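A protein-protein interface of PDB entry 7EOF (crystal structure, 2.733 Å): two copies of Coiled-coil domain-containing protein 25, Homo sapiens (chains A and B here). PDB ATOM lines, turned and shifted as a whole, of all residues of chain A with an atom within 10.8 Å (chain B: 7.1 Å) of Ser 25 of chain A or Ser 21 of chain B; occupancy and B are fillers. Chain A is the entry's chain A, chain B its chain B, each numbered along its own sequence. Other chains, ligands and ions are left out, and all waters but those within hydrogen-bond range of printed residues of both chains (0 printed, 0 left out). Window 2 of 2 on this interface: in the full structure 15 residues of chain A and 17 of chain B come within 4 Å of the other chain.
The side-chain hydroxyl of Ser 21 of chain B is in hydrogen-bond range of the side-chain hydroxyl of Ser 25 of chain A (3.1 Å).
The side-chain hydroxyl (OG1) of Thr 149 of chain B sits at hydrogen-bond distance from the backbone NH (N) of Thr 19 of chain B, 3.1 Å away. The side-chain hydroxyl (OG1) of Thr 149 of chain B is in hydrogen-bond range of the backbone carbonyl oxygen (O) of Leu 146 of chain B, at 2.8 Å. N of Thr 19 of chain A is in hydrogen-bond range of OG1 of Thr 149 of chain A. A ring nitrogen (NE2) of His 68 of chain A is in hydrogen-bond range of the backbone carbonyl oxygen (O) of Ala 27 of chain A, at 3.0 Å.
CG2 of Thr 149 of chain B touches O of Ser 25 of chain A (3.998 Å). Ala 27 of chain B touches Ala 27 of chain A. Ser 25 of chain B touches Arg 145 of chain A. Thr 149 of chain A touches Ser 25 of chain B (CG2 to O, 3.3 Å).
Asn 24 of chain A touches none of the printed residues of chain B. Of the printed residues of chain B, Ser 25 of chain A touches Ser 21 (3.1 Å) and Thr 149 (3.998 Å). Of the printed residues of chain B, Ala 27 of chain A touches Ala 27. Printed residues of chain B within 4 Å of Arg 145 of chain A: Ser 25. Of the printed residues of chain B, Thr 149 of chain A touches Ser 25 (3.3 Å). No residue of chain A comes within 4 Å of Thr 19 of chain B. No residue of chain A comes within 4 Å of Ser 20 of chain B. Ser 21 of chain B touches just one residue of chain A: Ser 25 (3.1 Å). No residue of chain A comes within 4 Å of Ser 22 of chain B. Of the printed residues of chain A, Ser 25 of chain B touches Arg 145 and Thr 149. Of chain A, only Ala 27 comes within 4 Å of Ala 27 of chain B. The nearest printed residue of chain B that does not touch Ser 25 of chain A is Arg 145 of chain B (4.7 Å). The nearest residue of chain A that does not touch Ser 21 of chain B is Ser 21 of chain A (4.7 Å). The nearest printed residue of chain B that does not touch Thr 149 of chain A is Ser 26 of chain B (5.2 Å).
Printed residues of chain A that touch a printed residue of chain B: Ser 25, Ala 27, Arg 145 and Thr 149. Hydrophobic or aromatic side chains of chain B that line the printed part of chain A: Ala 27. Along chain B the printed residues that touch a printed residue of chain A span positions 21 to 149. Among the printed residues, 5 pairs touch across the chains.
Ser 25 of chain A touches Ser 21 of chain B, but with the chains exchanged Ser 21 of chain A does not touch Ser 25 of chain B (4.6 Å). Ser 25 of chain A touches Thr 149 of chain B, and with the chains exchanged Thr 149 of chain A touches Ser 25 of chain B. Ala 27 of chain A touches its own counterpart, Ala 27 of chain B. Arg 145 of chain A touches Ser 25 of chain B, but with the chains exchanged Ser 25 of chain A does not touch Arg 145 of chain B (4.7 Å). Positions printed for both chains: 19, 20, 21, 22, 23, 24, 25, 26, 27, 28, 79, 80, 145 and 149. Of the 5 pairs that touch across the chains among the printed residues, 3 have their exchanged pair printed and touching as well.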
ATOM      1  N   THR A  19     -23.575 -14.237   7.160  1.00  0.00           N
ATOM      2  CA  THR A  19     -22.364 -14.822   7.715  1.00  0.00           C
ATOM      3  C   THR A  19     -22.611 -16.293   8.007  1.00  0.00           C
ATOM      4  O   THR A  19     -23.593 -16.641   8.673  1.00  0.00           O
ATOM      5  CB  THR A  19     -21.934 -14.087   8.985  1.00  0.00           C
ATOM      6  OG1 THR A  19     -21.799 -12.688   8.702  1.00  0.00           O
ATOM      7  CG2 THR A  19     -20.602 -14.627   9.488  1.00  0.00           C
ATOM      8  N   SER A  20     -21.728 -17.152   7.503  1.00  0.00           N
ATOM      9  CA  SER A  20     -21.801 -18.591   7.742  1.00  0.00           C
ATOM     10  C   SER A  20     -20.559 -19.014   8.514  1.00  0.00           C
ATOM     11  O   SER A  20     -19.444 -18.954   7.986  1.00  0.00           O
ATOM     12  CB  SER A  20     -21.916 -19.364   6.429  1.00  0.00           C
ATOM     13  OG  SER A  20     -22.050 -20.756   6.667  1.00  0.00           O
ATOM     14  N   SER A  21     -20.751 -19.434   9.760  1.00  0.00           N
ATOM     15  CA  SER A  21     -19.652 -19.955  10.560  1.00  0.00           C
ATOM     16  C   SER A  21     -19.438 -21.433  10.260  1.00  0.00           C
ATOM     17  O   SER A  21     -20.391 -22.177  10.009  1.00  0.00           O
ATOM     18  CB  SER A  21     -19.932 -19.752  12.048  1.00  0.00           C
ATOM     19  OG  SER A  21     -21.207 -20.264  12.397  1.00  0.00           O
ATOM     20  N   SER A  22     -18.178 -21.858  10.287  1.00  0.00           N
ATOM     21  CA  SER A  22     -17.825 -23.239  10.007  1.00  0.00           C
ATOM     22  C   SER A  22     -17.681 -24.020  11.313  1.00  0.00           C
ATOM     23  O   SER A  22     -17.802 -23.475  12.414  1.00  0.00           O
ATOM     24  CB  SER A  22     -16.539 -23.298   9.181  1.00  0.00           C
ATOM     25  OG  SER A  22     -16.196 -24.635   8.861  1.00  0.00           O
ATOM     26  N   VAL A  23     -17.414 -25.322  11.184  1.00  0.00           N
ATOM     27  CA  VAL A  23     -17.216 -26.161  12.362  1.00  0.00           C
ATOM     28  C   VAL A  23     -15.852 -25.928  12.998  1.00  0.00           C
ATOM     29  O   VAL A  23     -15.672 -26.216  14.187  1.00  0.00           O
ATOM     30  CB  VAL A  23     -17.401 -27.651  12.021  1.00  0.00           C
ATOM     31  CG1 VAL A  23     -18.783 -27.893  11.425  1.00  0.00           C
ATOM     32  CG2 VAL A  23     -16.307 -28.135  11.078  1.00  0.00           C
ATOM     33  N   ASN A  24     -14.888 -25.415  12.240  1.00  0.00           N
ATOM     34  CA  ASN A  24     -13.624 -24.942  12.785  1.00  0.00           C
ATOM     35  C   ASN A  24     -13.711 -23.499  13.264  1.00  0.00           C
ATOM     36  O   ASN A  24     -12.685 -22.919  13.633  1.00  0.00           O
ATOM     37  CB  ASN A  24     -12.506 -25.089  11.745  1.00  0.00           C
ATOM     38  CG  ASN A  24     -12.889 -24.527  10.390  1.00  0.00           C
ATOM     39  OD1 ASN A  24     -13.541 -23.490  10.294  1.00  0.00           O
ATOM     40  ND2 ASN A  24     -12.489 -25.222   9.329  1.00  0.00           N
ATOM     41  N   SER A  25     -14.910 -22.908  13.230  1.00  0.00           N
ATOM     42  CA  SER A  25     -15.165 -21.541  13.691  1.00  0.00           C
ATOM     43  C   SER A  25     -14.451 -20.511  12.816  1.00  0.00           C
ATOM     44  O   SER A  25     -13.949 -19.498  13.305  1.00  0.00           O
ATOM     45  CB  SER A  25     -14.785 -21.363  15.165  1.00  0.00           C
ATOM     46  OG  SER A  25     -15.272 -20.132  15.667  1.00  0.00           O
ATOM     47  N   SER A  26     -14.407 -20.773  11.514  1.00  0.00           N
ATOM     48  CA  SER A  26     -13.964 -19.804  10.523  1.00  0.00           C
ATOM     49  C   SER A  26     -15.189 -19.257   9.802  1.00  0.00           C
ATOM     50  O   SER A  26     -16.077 -20.023   9.410  1.00  0.00           O
ATOM     51  CB  SER A  26     -12.989 -20.435   9.528  1.00  0.00           C
ATOM     52  OG  SER A  26     -13.556 -21.580   8.917  1.00  0.00           O
ATOM     53  N   ALA A  27     -15.234 -17.941   9.632  1.00  0.00           N
ATOM     54  CA  ALA A  27     -16.410 -17.276   9.094  1.00  0.00           C
ATOM     55  C   ALA A  27     -16.291 -17.083   7.588  1.00  0.00           C
ATOM     56  O   ALA A  27     -15.200 -16.852   7.061  1.00  0.00           O
ATOM     57  CB  ALA A  27     -16.622 -15.924   9.774  1.00  0.00           C
ATOM     58  N   TYR A  28     -17.425 -17.195   6.900  1.00  0.00           N
ATOM     59  CA  TYR A  28     -17.514 -16.969   5.466  1.00  0.00           C
ATOM     60  C   TYR A  28     -18.613 -15.955   5.181  1.00  0.00           C
ATOM     61  O   TYR A  28     -19.684 -15.995   5.794  1.00  0.00           O
ATOM     62  CB  TYR A  28     -17.808 -18.267   4.710  1.00  0.00           C
ATOM     63  CG  TYR A  28     -16.679 -19.266   4.698  1.00  0.00           C
ATOM     64  CD1 TYR A  28     -16.498 -20.153   5.749  1.00  0.00           C
ATOM     65  CD2 TYR A  28     -15.805 -19.340   3.620  1.00  0.00           C
ATOM     66  CE1 TYR A  28     -15.471 -21.077   5.737  1.00  0.00           C
ATOM     67  CE2 TYR A  28     -14.774 -20.260   3.596  1.00  0.00           C
ATOM     68  CZ  TYR A  28     -14.611 -21.127   4.656  1.00  0.00           C
ATOM     69  OH  TYR A  28     -13.586 -22.043   4.633  1.00  0.00           O
ATOM     70  N   HIS A  68     -11.880 -17.541   1.584  1.00  0.00           N
ATOM     71  CA  HIS A  68     -10.652 -16.960   2.101  1.00  0.00           C
ATOM     72  C   HIS A  68      -9.586 -16.937   1.009  1.00  0.00           C
ATOM     73  O   HIS A  68      -9.616 -17.722   0.058  1.00  0.00           O
ATOM     74  CB  HIS A  68     -10.157 -17.743   3.316  1.00  0.00           C
ATOM     75  CG  HIS A  68     -11.118 -17.743   4.462  1.00  0.00           C
ATOM     76  ND1 HIS A  68     -11.981 -18.788   4.712  1.00  0.00           N
ATOM     77  CD2 HIS A  68     -11.358 -16.819   5.424  1.00  0.00           C
ATOM     78  CE1 HIS A  68     -12.707 -18.511   5.781  1.00  0.00           C
ATOM     79  NE2 HIS A  68     -12.348 -17.323   6.232  1.00  0.00           N
ATOM     80  N   GLU A  71      -8.075 -19.983  -0.800  1.00  0.00           N
ATOM     81  CA  GLU A  71      -8.944 -21.140  -0.656  1.00  0.00           C
ATOM     82  C   GLU A  71      -9.503 -21.547  -2.015  1.00  0.00           C
ATOM     83  O   GLU A  71      -9.752 -20.713  -2.888  1.00  0.00           O
ATOM     84  CB  GLU A  71     -10.081 -20.838   0.322  1.00  0.00           C
ATOM     85  CG  GLU A  71     -10.846 -22.064   0.806  1.00  0.00           C
ATOM     86  CD  GLU A  71     -11.760 -21.761   1.984  1.00  0.00           C
ATOM     87  OE1 GLU A  71     -11.809 -20.589   2.421  1.00  0.00           O
ATOM     88  OE2 GLU A  71     -12.427 -22.698   2.477  1.00  0.00           O
ATOM     89  N   PRO A  77     -15.983 -26.166   3.200  1.00  0.00           N
ATOM     90  CA  PRO A  77     -16.619 -27.053   4.177  1.00  0.00           C
ATOM     91  C   PRO A  77     -18.057 -27.347   3.780  1.00  0.00           C
ATOM     92  O   PRO A  77     -18.760 -26.492   3.238  1.00  0.00           O
ATOM     93  CB  PRO A  77     -16.553 -26.253   5.483  1.00  0.00           C
ATOM     94  CG  PRO A  77     -15.494 -25.219   5.257  1.00  0.00           C
ATOM     95  CD  PRO A  77     -15.543 -24.896   3.800  1.00  0.00           C
ATOM     96  N   GLU A  79     -20.710 -27.721   5.517  1.00  0.00           N
ATOM     97  CA  GLU A  79     -21.748 -26.949   6.193  1.00  0.00           C
ATOM     98  C   GLU A  79     -21.958 -25.597   5.521  1.00  0.00           C
ATOM     99  O   GLU A  79     -23.100 -25.161   5.336  1.00  0.00           O
ATOM    100  CB  GLU A  79     -21.407 -26.779   7.675  1.00  0.00           C
ATOM    101  CG  GLU A  79     -20.032 -26.185   7.968  1.00  0.00           C
ATOM    102  CD  GLU A  79     -18.907 -27.205   7.882  1.00  0.00           C
ATOM    103  OE1 GLU A  79     -19.120 -28.293   7.304  1.00  0.00           O
ATOM    104  OE2 GLU A  79     -17.806 -26.917   8.395  1.00  0.00           O
ATOM    105  N   VAL A  80     -20.869 -24.924   5.141  1.00  0.00           N
ATOM    106  CA  VAL A  80     -20.993 -23.661   4.421  1.00  0.00           C
ATOM    107  C   VAL A  80     -21.623 -23.892   3.053  1.00  0.00           C
ATOM    108  O   VAL A  80     -22.503 -23.134   2.619  1.00  0.00           O
ATOM    109  CB  VAL A  80     -19.615 -22.983   4.313  1.00  0.00           C
ATOM    110  CG1 VAL A  80     -19.727 -21.646   3.599  1.00  0.00           C
ATOM    111  CG2 VAL A  80     -19.006 -22.807   5.698  1.00  0.00           C
ATOM    112  N   ARG A 145     -31.070 -19.138  11.177  1.00  0.00           N
ATOM    113  CA  ARG A 145     -29.722 -18.839  11.653  1.00  0.00           C
ATOM    114  C   ARG A 145     -29.024 -17.849  10.726  1.00  0.00           C
ATOM    115  O   ARG A 145     -28.482 -16.835  11.179  1.00  0.00           O
ATOM    116  CB  ARG A 145     -28.920 -20.136  11.778  1.00  0.00           C
ATOM    117  CG  ARG A 145     -27.566 -19.994  12.454  1.00  0.00           C
ATOM    118  CD  ARG A 145     -26.456 -19.790  11.439  1.00  0.00           C
ATOM    119  NE  ARG A 145     -26.593 -20.694  10.300  1.00  0.00           N
ATOM    120  CZ  ARG A 145     -26.145 -21.945  10.279  1.00  0.00           C
ATOM    121  NH1 ARG A 145     -25.531 -22.449  11.340  1.00  0.00           N
ATOM    122  NH2 ARG A 145     -26.312 -22.695   9.196  1.00  0.00           N
ATOM    123  N   THR A 149     -28.007 -13.206  10.871  1.00  0.00           N
ATOM    124  CA  THR A 149     -26.792 -12.516  10.458  1.00  0.00           C
ATOM    125  C   THR A 149     -27.005 -11.625   9.242  1.00  0.00           C
ATOM    126  O   THR A 149     -26.056 -10.968   8.803  1.00  0.00           O
ATOM    127  CB  THR A 149     -25.671 -13.523  10.162  1.00  0.00           C
ATOM    128  OG1 THR A 149     -25.780 -13.983   8.809  1.00  0.00           O
ATOM    129  CG2 THR A 149     -25.757 -14.714  11.105  1.00  0.00           C
ATOM    130  N   THR B  19     -10.299 -13.844  13.534  1.00  0.00           N
ATOM    131  CA  THR B  19     -11.751 -13.861  13.606  1.00  0.00           C
ATOM    132  C   THR B  19     -12.176 -14.467  14.934  1.00  0.00           C
ATOM    133  O   THR B  19     -11.625 -15.488  15.360  1.00  0.00           O
ATOM    134  CB  THR B  19     -12.354 -14.648  12.438  1.00  0.00           C
ATOM    135  OG1 THR B  19     -11.900 -14.081  11.202  1.00  0.00           O
ATOM    136  CG2 THR B  19     -13.870 -14.587  12.482  1.00  0.00           C
ATOM    137  N   SER B  20     -13.141 -13.825  15.592  1.00  0.00           N
ATOM    138  CA  SER B  20     -13.697 -14.282  16.861  1.00  0.00           C
ATOM    139  C   SER B  20     -15.195 -14.501  16.683  1.00  0.00           C
ATOM    140  O   SER B  20     -15.949 -13.541  16.491  1.00  0.00           O
ATOM    141  CB  SER B  20     -13.417 -13.271  17.974  1.00  0.00           C
ATOM    142  OG  SER B  20     -14.042 -13.651  19.188  1.00  0.00           O
ATOM    143  N   SER B  21     -15.624 -15.758  16.742  1.00  0.00           N
ATOM    144  CA  SER B  21     -17.044 -16.071  16.721  1.00  0.00           C
ATOM    145  C   SER B  21     -17.628 -15.957  18.124  1.00  0.00           C
ATOM    146  O   SER B  21     -16.956 -16.229  19.123  1.00  0.00           O
ATOM    147  CB  SER B  21     -17.279 -17.479  16.168  1.00  0.00           C
ATOM    148  OG  SER B  21     -16.815 -17.597  14.831  1.00  0.00           O
ATOM    149  N   SER B  22     -18.889 -15.543  18.193  1.00  0.00           N
ATOM    150  CA  SER B  22     -19.616 -15.436  19.452  1.00  0.00           C
ATOM    151  C   SER B  22     -20.796 -16.405  19.448  1.00  0.00           C
ATOM    152  O   SER B  22     -21.069 -17.088  18.457  1.00  0.00           O
ATOM    153  CB  SER B  22     -20.096 -14.001  19.686  1.00  0.00           C
ATOM    154  OG  SER B  22     -21.103 -13.643  18.755  1.00  0.00           O
ATOM    155  N   VAL B  23     -21.509 -16.450  20.577  1.00  0.00           N
ATOM    156  CA  VAL B  23     -22.706 -17.277  20.682  1.00  0.00           C
ATOM    157  C   VAL B  23     -23.883 -16.683  19.928  1.00  0.00           C
ATOM    158  O   VAL B  23     -24.881 -17.375  19.701  1.00  0.00           O
ATOM    159  CB  VAL B  23     -23.091 -17.493  22.160  1.00  0.00           C
ATOM    160  CG1 VAL B  23     -21.928 -18.106  22.926  1.00  0.00           C
ATOM    161  CG2 VAL B  23     -23.526 -16.180  22.794  1.00  0.00           C
ATOM    162  N   ASN B  24     -23.784 -15.413  19.533  1.00  0.00           N
ATOM    163  CA  ASN B  24     -24.789 -14.739  18.721  1.00  0.00           C
ATOM    164  C   ASN B  24     -24.798 -15.214  17.276  1.00  0.00           C
ATOM    165  O   ASN B  24     -25.631 -14.735  16.499  1.00  0.00           O
ATOM    166  CB  ASN B  24     -24.563 -13.226  18.761  1.00  0.00           C
ATOM    167  N   SER B  25     -23.881 -16.111  16.902  1.00  0.00           N
ATOM    168  CA  SER B  25     -23.699 -16.553  15.517  1.00  0.00           C
ATOM    169  C   SER B  25     -23.236 -15.403  14.629  1.00  0.00           C
ATOM    170  O   SER B  25     -23.487 -15.392  13.422  1.00  0.00           O
ATOM    171  CB  SER B  25     -24.971 -17.200  14.954  1.00  0.00           C
ATOM    172  OG  SER B  25     -24.768 -17.686  13.637  1.00  0.00           O
ATOM    173  N   SER B  26     -22.557 -14.429  15.230  1.00  0.00           N
ATOM    174  CA  SER B  26     -21.971 -13.303  14.520  1.00  0.00           C
ATOM    175  C   SER B  26     -20.472 -13.291  14.772  1.00  0.00           C
ATOM    176  O   SER B  26     -20.032 -13.405  15.921  1.00  0.00           O
ATOM    177  CB  SER B  26     -22.597 -11.983  14.973  1.00  0.00           C
ATOM    178  OG  SER B  26     -22.506 -11.845  16.381  1.00  0.00           O
ATOM    179  N   ALA B  27     -19.693 -13.151  13.706  1.00  0.00           N
ATOM    180  CA  ALA B  27     -18.243 -13.171  13.802  1.00  0.00           C
ATOM    181  C   ALA B  27     -17.689 -11.754  13.753  1.00  0.00           C
ATOM    182  O   ALA B  27     -18.234 -10.877  13.080  1.00  0.00           O
ATOM    183  CB  ALA B  27     -17.627 -14.009  12.682  1.00  0.00           C
ATOM    184  N   TYR B  28     -16.601 -11.540  14.485  1.00  0.00           N
ATOM    185  CA  TYR B  28     -15.945 -10.245  14.566  1.00  0.00           C
ATOM    186  C   TYR B  28     -14.524 -10.353  14.037  1.00  0.00           C
ATOM    187  O   TYR B  28     -13.846 -11.360  14.259  1.00  0.00           O
ATOM    188  CB  TYR B  28     -15.931  -9.734  16.005  1.00  0.00           C
ATOM    189  CG  TYR B  28     -17.301  -9.415  16.555  1.00  0.00           C
ATOM    190  CD1 TYR B  28     -18.102 -10.408  17.101  1.00  0.00           C
ATOM    191  CD2 TYR B  28     -17.790  -8.116  16.536  1.00  0.00           C
ATOM    192  CE1 TYR B  28     -19.352 -10.117  17.609  1.00  0.00           C
ATOM    193  CE2 TYR B  28     -19.037  -7.815  17.041  1.00  0.00           C
ATOM    194  CZ  TYR B  28     -19.815  -8.816  17.575  1.00  0.00           C
ATOM    195  OH  TYR B  28     -21.060  -8.512  18.078  1.00  0.00           O
ATOM    196  N   GLU B  79     -17.274 -12.513  25.638  1.00  0.00           N
ATOM    197  CA  GLU B  79     -16.295 -13.488  25.165  1.00  0.00           C
ATOM    198  C   GLU B  79     -15.365 -12.887  24.115  1.00  0.00           C
ATOM    199  O   GLU B  79     -14.163 -13.174  24.112  1.00  0.00           O
ATOM    200  CB  GLU B  79     -16.997 -14.735  24.620  1.00  0.00           C
ATOM    201  CG  GLU B  79     -17.981 -14.491  23.483  1.00  0.00           C
ATOM    202  CD  GLU B  79     -19.369 -14.121  23.969  1.00  0.00           C
ATOM    203  OE1 GLU B  79     -19.508 -13.753  25.155  1.00  0.00           O
ATOM    204  OE2 GLU B  79     -20.322 -14.206  23.164  1.00  0.00           O
ATOM    205  N   VAL B  80     -15.896 -12.048  23.221  1.00  0.00           N
ATOM    206  CA  VAL B  80     -15.056 -11.413  22.210  1.00  0.00           C
ATOM    207  C   VAL B  80     -14.142 -10.379  22.851  1.00  0.00           C
ATOM    208  O   VAL B  80     -12.975 -10.229  22.461  1.00  0.00           O
ATOM    209  CB  VAL B  80     -15.930 -10.787  21.110  1.00  0.00           C
ATOM    210  CG1 VAL B  80     -15.059 -10.196  20.012  1.00  0.00           C
ATOM    211  CG2 VAL B  80     -16.882 -11.821  20.546  1.00  0.00           C
ATOM    212  N   ASP B  83     -11.436 -12.203  24.322  1.00  0.00           N
ATOM    213  CA  ASP B  83     -10.553 -12.656  23.253  1.00  0.00           C
ATOM    214  C   ASP B  83      -9.556 -11.567  22.879  1.00  0.00           C
ATOM    215  O   ASP B  83      -8.350 -11.823  22.786  1.00  0.00           O
ATOM    216  CB  ASP B  83     -11.371 -13.086  22.036  1.00  0.00           C
ATOM    217  CG  ASP B  83     -11.957 -14.473  22.192  1.00  0.00           C
ATOM    218  OD1 ASP B  83     -12.105 -14.927  23.347  1.00  0.00           O
ATOM    219  OD2 ASP B  83     -12.263 -15.110  21.161  1.00  0.00           O
ATOM    220  N   ARG B 145      -7.515 -21.144  19.477  1.00  0.00           N
ATOM    221  CA  ARG B 145      -8.645 -20.883  18.589  1.00  0.00           C
ATOM    222  C   ARG B 145      -8.397 -19.652  17.728  1.00  0.00           C
ATOM    223  O   ARG B 145      -8.661 -19.668  16.519  1.00  0.00           O
ATOM    224  CB  ARG B 145      -9.933 -20.716  19.394  1.00  0.00           C
ATOM    225  CG  ARG B 145     -11.171 -20.565  18.521  1.00  0.00           C
ATOM    226  CD  ARG B 145     -12.420 -20.304  19.340  1.00  0.00           C
ATOM    227  NE  ARG B 145     -12.333 -19.051  20.082  1.00  0.00           N
ATOM    228  CZ  ARG B 145     -12.101 -18.972  21.388  1.00  0.00           C
ATOM    229  NH1 ARG B 145     -11.939 -20.079  22.103  1.00  0.00           N
ATOM    230  NH2 ARG B 145     -12.039 -17.788  21.980  1.00  0.00           N
ATOM    231  N   LEU B 146      -7.882 -18.577  18.330  1.00  0.00           N
ATOM    232  CA  LEU B 146      -7.586 -17.378  17.552  1.00  0.00           C
ATOM    233  C   LEU B 146      -6.463 -17.631  16.554  1.00  0.00           C
ATOM    234  O   LEU B 146      -6.478 -17.089  15.444  1.00  0.00           O
ATOM    235  CB  LEU B 146      -7.224 -16.225  18.486  1.00  0.00           C
ATOM    236  CG  LEU B 146      -8.271 -15.867  19.541  1.00  0.00           C
ATOM    237  CD1 LEU B 146      -7.754 -14.765  20.453  1.00  0.00           C
ATOM    238  CD2 LEU B 146      -9.585 -15.462  18.886  1.00  0.00           C
ATOM    239  N   LYS B 148      -5.849 -20.381  14.979  1.00  0.00           N
ATOM    240  CA  LYS B 148      -6.366 -21.098  13.817  1.00  0.00           C
ATOM    241  C   LYS B 148      -6.860 -20.138  12.741  1.00  0.00           C
ATOM    242  O   LYS B 148      -6.761 -20.443  11.546  1.00  0.00           O
ATOM    243  CB  LYS B 148      -7.487 -22.054  14.232  1.00  0.00           C
ATOM    244  CG  LYS B 148      -7.000 -23.424  14.688  1.00  0.00           C
ATOM    245  CD  LYS B 148      -8.160 -24.391  14.886  1.00  0.00           C
ATOM    246  CE  LYS B 148      -7.666 -25.787  15.232  1.00  0.00           C
ATOM    247  NZ  LYS B 148      -8.793 -26.733  15.457  1.00  0.00           N
ATOM    248  N   THR B 149      -7.375 -18.976  13.138  1.00  0.00           N
ATOM    249  CA  THR B 149      -7.920 -17.997  12.207  1.00  0.00           C
ATOM    250  C   THR B 149      -6.911 -16.930  11.797  1.00  0.00           C
ATOM    251  O   THR B 149      -7.274 -16.014  11.053  1.00  0.00           O
ATOM    252  CB  THR B 149      -9.145 -17.314  12.818  1.00  0.00           C
ATOM    253  OG1 THR B 149      -8.729 -16.467  13.897  1.00  0.00           O
ATOM    254  CG2 THR B 149     -10.120 -18.350  13.347  1.00  0.00           C
